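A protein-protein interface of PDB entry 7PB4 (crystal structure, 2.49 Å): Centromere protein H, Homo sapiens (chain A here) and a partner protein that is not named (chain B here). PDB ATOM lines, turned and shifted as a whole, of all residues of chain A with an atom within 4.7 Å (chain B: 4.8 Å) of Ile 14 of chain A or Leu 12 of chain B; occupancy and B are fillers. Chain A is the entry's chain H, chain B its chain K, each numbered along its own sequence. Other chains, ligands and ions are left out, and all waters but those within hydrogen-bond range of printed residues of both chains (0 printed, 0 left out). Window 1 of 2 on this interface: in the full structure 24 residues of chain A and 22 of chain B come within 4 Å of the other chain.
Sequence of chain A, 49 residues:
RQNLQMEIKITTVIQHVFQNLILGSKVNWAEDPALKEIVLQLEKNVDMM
The side-chain amide nitrogen (NE2) of Gln 15 of chain A is in hydrogen-bond range of the side-chain hydroxyl (OH) of Tyr 8 of chain B, 2.9 Å away.
The backbone carbonyl oxygen of Lys 11 of chain B is in hydrogen-bond range of the side-chain hydroxyl of Thr 15 of chain B, at 3.0 Å.
The backbone carbonyl oxygen (O) of Leu 12 of chain B is in hydrogen-bond range of the side-chain hydroxyl (OG1) of Thr 15 of chain B (3.0 Å).
Ile 10 of chain A touches Lys 9 of chain B (CG2 to NZ, 3.8 Å).
Tyr 8 of chain B touches Thr 11 of chain A.
Thr 11 of chain A touches Lys 9 of chain B.
Ile 14 of chain A touches Leu 12 of chain B (CG2 to CD2, 3.7 Å).
Leu 13 of chain B touches Ile 14 of chain A (CD2 to CD1, 3.6 Å).
CG of Gln 15 of chain A touches CD2 of Leu 12 of chain B, 3.6 Å away.
CE2 of Phe 18 of chain A touches OG1 of Thr 15 of chain B, at 3.5 Å.
CD1 of Leu 16 of chain B touches CD1 of Phe 18 of chain A (3.6 Å).
Thr 15 of chain B touches Ile 38 of chain A.
Leu 42 of chain A touches Tyr 8 of chain B.
Ile 14 of chain A touches two residues of chain B.
Of the printed residues of chain B, Gln 15 of chain A touches Tyr 8 (2.9 Å) and Leu 12 (3.6 Å).
Printed residues of chain A within 4 Å of Leu 13 of chain B: Ile 14.
Of the printed residues of chain B, Thr 11 of chain A touches Tyr 8 (3.6 Å) and Lys 9 (3.7 Å).
Printed residues of chain B within 4 Å of Ile 10 of chain A: Lys 9.
Ile 56 of chain B touches none of the printed residues of chain A.
His 16 of chain A touches none of the printed residues of chain B.
Of the 10 printed residues of chain B, 6 touch a printed residue of chain A.
Hydrophobic or aromatic side chains of chain B within 4 Å of the printed part of chain A: Tyr 8, Leu 12, Leu 13 and Leu 16.
Along chain B the printed residues that touch a printed residue of chain A span positions 8 to 16.
Among the printed residues, 12 pairs touch across the chains.
Among the printed residues, no Asp or Glu carboxylate lies within 4 Å of a Lys or Arg side-chain nitrogen of the other chain.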
ATOM      1  N   ILE A  10      12.292  19.153 -27.356  1.00  0.00           N
ATOM      2  CA  ILE A  10      12.885  18.463 -26.215  1.00  0.00           C
ATOM      3  C   ILE A  10      13.827  19.392 -25.458  1.00  0.00           C
ATOM      4  O   ILE A  10      13.864  19.385 -24.223  1.00  0.00           O
ATOM      5  CB  ILE A  10      13.601  17.181 -26.684  1.00  0.00           C
ATOM      6  CG1 ILE A  10      12.581  16.147 -27.167  1.00  0.00           C
ATOM      7  CG2 ILE A  10      14.457  16.598 -25.572  1.00  0.00           C
ATOM      8  CD1 ILE A  10      13.208  14.923 -27.798  1.00  0.00           C
ATOM      9  N   THR A  11      14.591  20.212 -26.181  1.00  0.00           N
ATOM     10  CA  THR A  11      15.508  21.136 -25.520  1.00  0.00           C
ATOM     11  C   THR A  11      14.749  22.205 -24.743  1.00  0.00           C
ATOM     12  O   THR A  11      15.174  22.605 -23.653  1.00  0.00           O
ATOM     13  CB  THR A  11      16.438  21.776 -26.550  1.00  0.00           C
ATOM     14  OG1 THR A  11      17.033  20.752 -27.356  1.00  0.00           O
ATOM     15  CG2 THR A  11      17.538  22.563 -25.854  1.00  0.00           C
ATOM     16  N   THR A  12      13.623  22.676 -25.284  1.00  0.00           N
ATOM     17  CA  THR A  12      12.783  23.608 -24.533  1.00  0.00           C
ATOM     18  C   THR A  12      12.256  22.962 -23.253  1.00  0.00           C
ATOM     19  O   THR A  12      12.276  23.576 -22.173  1.00  0.00           O
ATOM     20  CB  THR A  12      11.624  24.087 -25.408  1.00  0.00           C
ATOM     21  OG1 THR A  12      12.141  24.688 -26.603  1.00  0.00           O
ATOM     22  CG2 THR A  12      10.773  25.104 -24.661  1.00  0.00           C
ATOM     23  N   VAL A  13      11.782  21.718 -23.361  1.00  0.00           N
ATOM     24  CA  VAL A  13      11.290  21.000 -22.187  1.00  0.00           C
ATOM     25  C   VAL A  13      12.396  20.846 -21.150  1.00  0.00           C
ATOM     26  O   VAL A  13      12.166  21.007 -19.946  1.00  0.00           O
ATOM     27  CB  VAL A  13      10.706  19.637 -22.604  1.00  0.00           C
ATOM     28  CG1 VAL A  13      10.359  18.806 -21.378  1.00  0.00           C
ATOM     29  CG2 VAL A  13       9.480  19.832 -23.480  1.00  0.00           C
ATOM     30  N   ILE A  14      13.615  20.540 -21.601  1.00  0.00           N
ATOM     31  CA  ILE A  14      14.731  20.360 -20.677  1.00  0.00           C
ATOM     32  C   ILE A  14      15.089  21.678 -20.004  1.00  0.00           C
ATOM     33  O   ILE A  14      15.384  21.714 -18.803  1.00  0.00           O
ATOM     34  CB  ILE A  14      15.939  19.748 -21.409  1.00  0.00           C
ATOM     35  CG1 ILE A  14      15.611  18.337 -21.897  1.00  0.00           C
ATOM     36  CG2 ILE A  14      17.157  19.709 -20.499  1.00  0.00           C
ATOM     37  CD1 ILE A  14      16.639  17.769 -22.849  1.00  0.00           C
ATOM     38  N   GLN A  15      15.080  22.778 -20.764  1.00  0.00           N
ATOM     39  CA  GLN A  15      15.286  24.098 -20.176  1.00  0.00           C
ATOM     40  C   GLN A  15      14.305  24.349 -19.039  1.00  0.00           C
ATOM     41  O   GLN A  15      14.698  24.724 -17.925  1.00  0.00           O
ATOM     42  CB  GLN A  15      15.128  25.185 -21.242  1.00  0.00           C
ATOM     43  CG  GLN A  15      16.298  25.348 -22.188  1.00  0.00           C
ATOM     44  CD  GLN A  15      16.072  26.477 -23.174  1.00  0.00           C
ATOM     45  OE1 GLN A  15      14.933  26.861 -23.444  1.00  0.00           O
ATOM     46  NE2 GLN A  15      17.157  27.021 -23.711  1.00  0.00           N
ATOM     47  N   HIS A  16      13.013  24.145 -19.310  1.00  0.00           N
ATOM     48  CA  HIS A  16      12.002  24.438 -18.297  1.00  0.00           C
ATOM     49  C   HIS A  16      12.133  23.514 -17.090  1.00  0.00           C
ATOM     50  O   HIS A  16      11.977  23.953 -15.943  1.00  0.00           O
ATOM     51  CB  HIS A  16      10.605  24.337 -18.902  1.00  0.00           C
ATOM     52  CG  HIS A  16      10.170  25.571 -19.629  1.00  0.00           C
ATOM     53  ND1 HIS A  16      10.610  25.886 -20.896  1.00  0.00           N
ATOM     54  CD2 HIS A  16       9.330  26.568 -19.263  1.00  0.00           C
ATOM     55  CE1 HIS A  16      10.061  27.024 -21.279  1.00  0.00           C
ATOM     56  NE2 HIS A  16       9.280  27.459 -20.307  1.00  0.00           N
ATOM     57  N   VAL A  17      12.418  22.230 -17.326  1.00  0.00           N
ATOM     58  CA  VAL A  17      12.558  21.287 -16.218  1.00  0.00           C
ATOM     59  C   VAL A  17      13.751  21.658 -15.348  1.00  0.00           C
ATOM     60  O   VAL A  17      13.667  21.641 -14.113  1.00  0.00           O
ATOM     61  CB  VAL A  17      12.669  19.846 -16.753  1.00  0.00           C
ATOM     62  CG1 VAL A  17      13.114  18.897 -15.650  1.00  0.00           C
ATOM     63  CG2 VAL A  17      11.340  19.394 -17.334  1.00  0.00           C
ATOM     64  N   PHE A  18      14.878  22.005 -15.977  1.00  0.00           N
ATOM     65  CA  PHE A  18      16.055  22.419 -15.221  1.00  0.00           C
ATOM     66  C   PHE A  18      15.764  23.667 -14.399  1.00  0.00           C
ATOM     67  O   PHE A  18      16.144  23.749 -13.223  1.00  0.00           O
ATOM     68  CB  PHE A  18      17.225  22.662 -16.177  1.00  0.00           C
ATOM     69  CG  PHE A  18      18.580  22.539 -15.535  1.00  0.00           C
ATOM     70  CD1 PHE A  18      18.710  22.324 -14.172  1.00  0.00           C
ATOM     71  CD2 PHE A  18      19.730  22.643 -16.301  1.00  0.00           C
ATOM     72  CE1 PHE A  18      19.957  22.212 -13.586  1.00  0.00           C
ATOM     73  CE2 PHE A  18      20.981  22.532 -15.722  1.00  0.00           C
ATOM     74  CZ  PHE A  18      21.093  22.317 -14.362  1.00  0.00           C
ATOM     75  N   ILE A  38      25.376  28.470 -15.981  1.00  0.00           N
ATOM     76  CA  ILE A  38      24.390  27.644 -16.676  1.00  0.00           C
ATOM     77  C   ILE A  38      22.984  28.217 -16.535  1.00  0.00           C
ATOM     78  O   ILE A  38      22.175  28.126 -17.462  1.00  0.00           O
ATOM     79  CB  ILE A  38      24.471  26.195 -16.156  1.00  0.00           C
ATOM     80  CG1 ILE A  38      25.798  25.562 -16.573  1.00  0.00           C
ATOM     81  CG2 ILE A  38      23.307  25.361 -16.671  1.00  0.00           C
ATOM     82  CD1 ILE A  38      26.221  24.420 -15.689  1.00  0.00           C
ATOM     83  N   LEU A  42      20.027  29.343 -19.681  1.00  0.00           N
ATOM     84  CA  LEU A  42      18.597  29.175 -19.870  1.00  0.00           C
ATOM     85  C   LEU A  42      17.982  30.464 -20.415  1.00  0.00           C
ATOM     86  O   LEU A  42      18.645  31.500 -20.536  1.00  0.00           O
ATOM     87  CB  LEU A  42      17.929  28.771 -18.557  1.00  0.00           C
ATOM     88  CG  LEU A  42      18.433  27.467 -17.933  1.00  0.00           C
ATOM     89  CD1 LEU A  42      17.789  27.236 -16.577  1.00  0.00           C
ATOM     90  CD2 LEU A  42      18.169  26.291 -18.860  1.00  0.00           C
ATOM     91  N   TYR B   8      24.065  22.395 -27.329  1.00  0.00           N
ATOM     92  CA  TYR B   8      23.390  22.995 -26.200  1.00  0.00           C
ATOM     93  C   TYR B   8      22.626  21.968 -25.443  1.00  0.00           C
ATOM     94  O   TYR B   8      22.659  21.935 -24.239  1.00  0.00           O
ATOM     95  CB  TYR B   8      22.458  24.122 -26.655  1.00  0.00           C
ATOM     96  CG  TYR B   8      21.758  24.868 -25.570  1.00  0.00           C
ATOM     97  CD1 TYR B   8      22.428  25.785 -24.789  1.00  0.00           C
ATOM     98  CD2 TYR B   8      20.415  24.674 -25.343  1.00  0.00           C
ATOM     99  CE1 TYR B   8      21.779  26.472 -23.792  1.00  0.00           C
ATOM    100  CE2 TYR B   8      19.762  25.353 -24.349  1.00  0.00           C
ATOM    101  CZ  TYR B   8      20.449  26.251 -23.582  1.00  0.00           C
ATOM    102  OH  TYR B   8      19.787  26.924 -22.599  1.00  0.00           O
ATOM    103  N   LYS B   9      21.926  21.131 -26.177  1.00  0.00           N
ATOM    104  CA  LYS B   9      21.131  20.107 -25.512  1.00  0.00           C
ATOM    105  C   LYS B   9      22.007  19.156 -24.707  1.00  0.00           C
ATOM    106  O   LYS B   9      21.672  18.820 -23.566  1.00  0.00           O
ATOM    107  CB  LYS B   9      20.310  19.334 -26.545  1.00  0.00           C
ATOM    108  CG  LYS B   9      19.561  18.139 -25.976  1.00  0.00           C
ATOM    109  CD  LYS B   9      18.839  17.367 -27.068  1.00  0.00           C
ATOM    110  CE  LYS B   9      18.172  16.120 -26.511  1.00  0.00           C
ATOM    111  NZ  LYS B   9      17.478  15.337 -27.570  1.00  0.00           N
ATOM    112  N   GLU B  10      23.132  18.714 -25.277  1.00  0.00           N
ATOM    113  CA  GLU B  10      23.996  17.789 -24.551  1.00  0.00           C
ATOM    114  C   GLU B  10      24.627  18.456 -23.334  1.00  0.00           C
ATOM    115  O   GLU B  10      24.718  17.842 -22.262  1.00  0.00           O
ATOM    116  CB  GLU B  10      25.070  17.226 -25.482  1.00  0.00           C
ATOM    117  CG  GLU B  10      24.538  16.220 -26.493  1.00  0.00           C
ATOM    118  CD  GLU B  10      25.643  15.439 -27.180  1.00  0.00           C
ATOM    119  OE1 GLU B  10      26.824  15.807 -27.018  1.00  0.00           O
ATOM    120  OE2 GLU B  10      25.329  14.452 -27.880  1.00  0.00           O
ATOM    121  N   LYS B  11      25.060  19.712 -23.472  1.00  0.00           N
ATOM    122  CA  LYS B  11      25.603  20.433 -22.323  1.00  0.00           C
ATOM    123  C   LYS B  11      24.552  20.587 -21.230  1.00  0.00           C
ATOM    124  O   LYS B  11      24.819  20.327 -20.048  1.00  0.00           O
ATOM    125  CB  LYS B  11      26.125  21.802 -22.759  1.00  0.00           C
ATOM    126  CG  LYS B  11      26.654  22.652 -21.614  1.00  0.00           C
ATOM    127  CD  LYS B  11      26.768  24.113 -22.014  1.00  0.00           C
ATOM    128  CE  LYS B  11      25.402  24.710 -22.315  1.00  0.00           C
ATOM    129  NZ  LYS B  11      25.488  26.152 -22.676  1.00  0.00           N
ATOM    130  N   LEU B  12      23.346  21.016 -21.614  1.00  0.00           N
ATOM    131  CA  LEU B  12      22.266  21.191 -20.651  1.00  0.00           C
ATOM    132  C   LEU B  12      21.944  19.881 -19.946  1.00  0.00           C
ATOM    133  O   LEU B  12      21.745  19.857 -18.728  1.00  0.00           O
ATOM    134  CB  LEU B  12      21.028  21.738 -21.364  1.00  0.00           C
ATOM    135  CG  LEU B  12      20.042  22.585 -20.559  1.00  0.00           C
ATOM    136  CD1 LEU B  12      20.698  23.882 -20.118  1.00  0.00           C
ATOM    137  CD2 LEU B  12      18.800  22.863 -21.386  1.00  0.00           C
ATOM    138  N   LEU B  13      21.920  18.775 -20.694  1.00  0.00           N
ATOM    139  CA  LEU B  13      21.589  17.481 -20.107  1.00  0.00           C
ATOM    140  C   LEU B  13      22.664  17.011 -19.136  1.00  0.00           C
ATOM    141  O   LEU B  13      22.347  16.523 -18.046  1.00  0.00           O
ATOM    142  CB  LEU B  13      21.378  16.451 -21.213  1.00  0.00           C
ATOM    143  CG  LEU B  13      19.977  16.353 -21.815  1.00  0.00           C
ATOM    144  CD1 LEU B  13      19.967  15.370 -22.972  1.00  0.00           C
ATOM    145  CD2 LEU B  13      18.977  15.937 -20.750  1.00  0.00           C
ATOM    146  N   SER B  14      23.940  17.139 -19.513  1.00  0.00           N
ATOM    147  CA  SER B  14      25.007  16.716 -18.613  1.00  0.00           C
ATOM    148  C   SER B  14      25.001  17.538 -17.330  1.00  0.00           C
ATOM    149  O   SER B  14      25.094  16.983 -16.225  1.00  0.00           O
ATOM    150  CB  SER B  14      26.363  16.820 -19.310  1.00  0.00           C
ATOM    151  OG  SER B  14      26.683  18.168 -19.606  1.00  0.00           O
ATOM    152  N   THR B  15      24.888  18.863 -17.454  1.00  0.00           N
ATOM    153  CA  THR B  15      24.869  19.702 -16.263  1.00  0.00           C
ATOM    154  C   THR B  15      23.629  19.444 -15.415  1.00  0.00           C
ATOM    155  O   THR B  15      23.714  19.465 -14.182  1.00  0.00           O
ATOM    156  CB  THR B  15      24.963  21.173 -16.661  1.00  0.00           C
ATOM    157  OG1 THR B  15      23.836  21.526 -17.470  1.00  0.00           O
ATOM    158  CG2 THR B  15      26.245  21.419 -17.448  1.00  0.00           C
ATOM    159  N   LEU B  16      22.484  19.168 -16.047  1.00  0.00           N
ATOM    160  CA  LEU B  16      21.280  18.826 -15.297  1.00  0.00           C
ATOM    161  C   LEU B  16      21.457  17.519 -14.539  1.00  0.00           C
ATOM    162  O   LEU B  16      21.022  17.401 -13.389  1.00  0.00           O
ATOM    163  CB  LEU B  16      20.082  18.743 -16.244  1.00  0.00           C
ATOM    164  CG  LEU B  16      18.822  18.049 -15.715  1.00  0.00           C
ATOM    165  CD1 LEU B  16      18.210  18.819 -14.554  1.00  0.00           C
ATOM    166  CD2 LEU B  16      17.801  17.848 -16.828  1.00  0.00           C
ATOM    167  N   ILE B  56       9.979  12.328 -20.219  1.00  0.00           N
ATOM    168  CA  ILE B  56      10.265  13.049 -21.458  1.00  0.00           C
ATOM    169  C   ILE B  56      10.056  12.143 -22.666  1.00  0.00           C
ATOM    170  O   ILE B  56       9.538  12.576 -23.703  1.00  0.00           O
ATOM    171  CB  ILE B  56      11.692  13.626 -21.424  1.00  0.00           C
ATOM    172  CG1 ILE B  56      11.821  14.668 -20.312  1.00  0.00           C
ATOM    173  CG2 ILE B  56      12.055  14.243 -22.766  1.00  0.00           C
ATOM    174  CD1 ILE B  56      13.232  15.172 -20.108  1.00  0.00           C
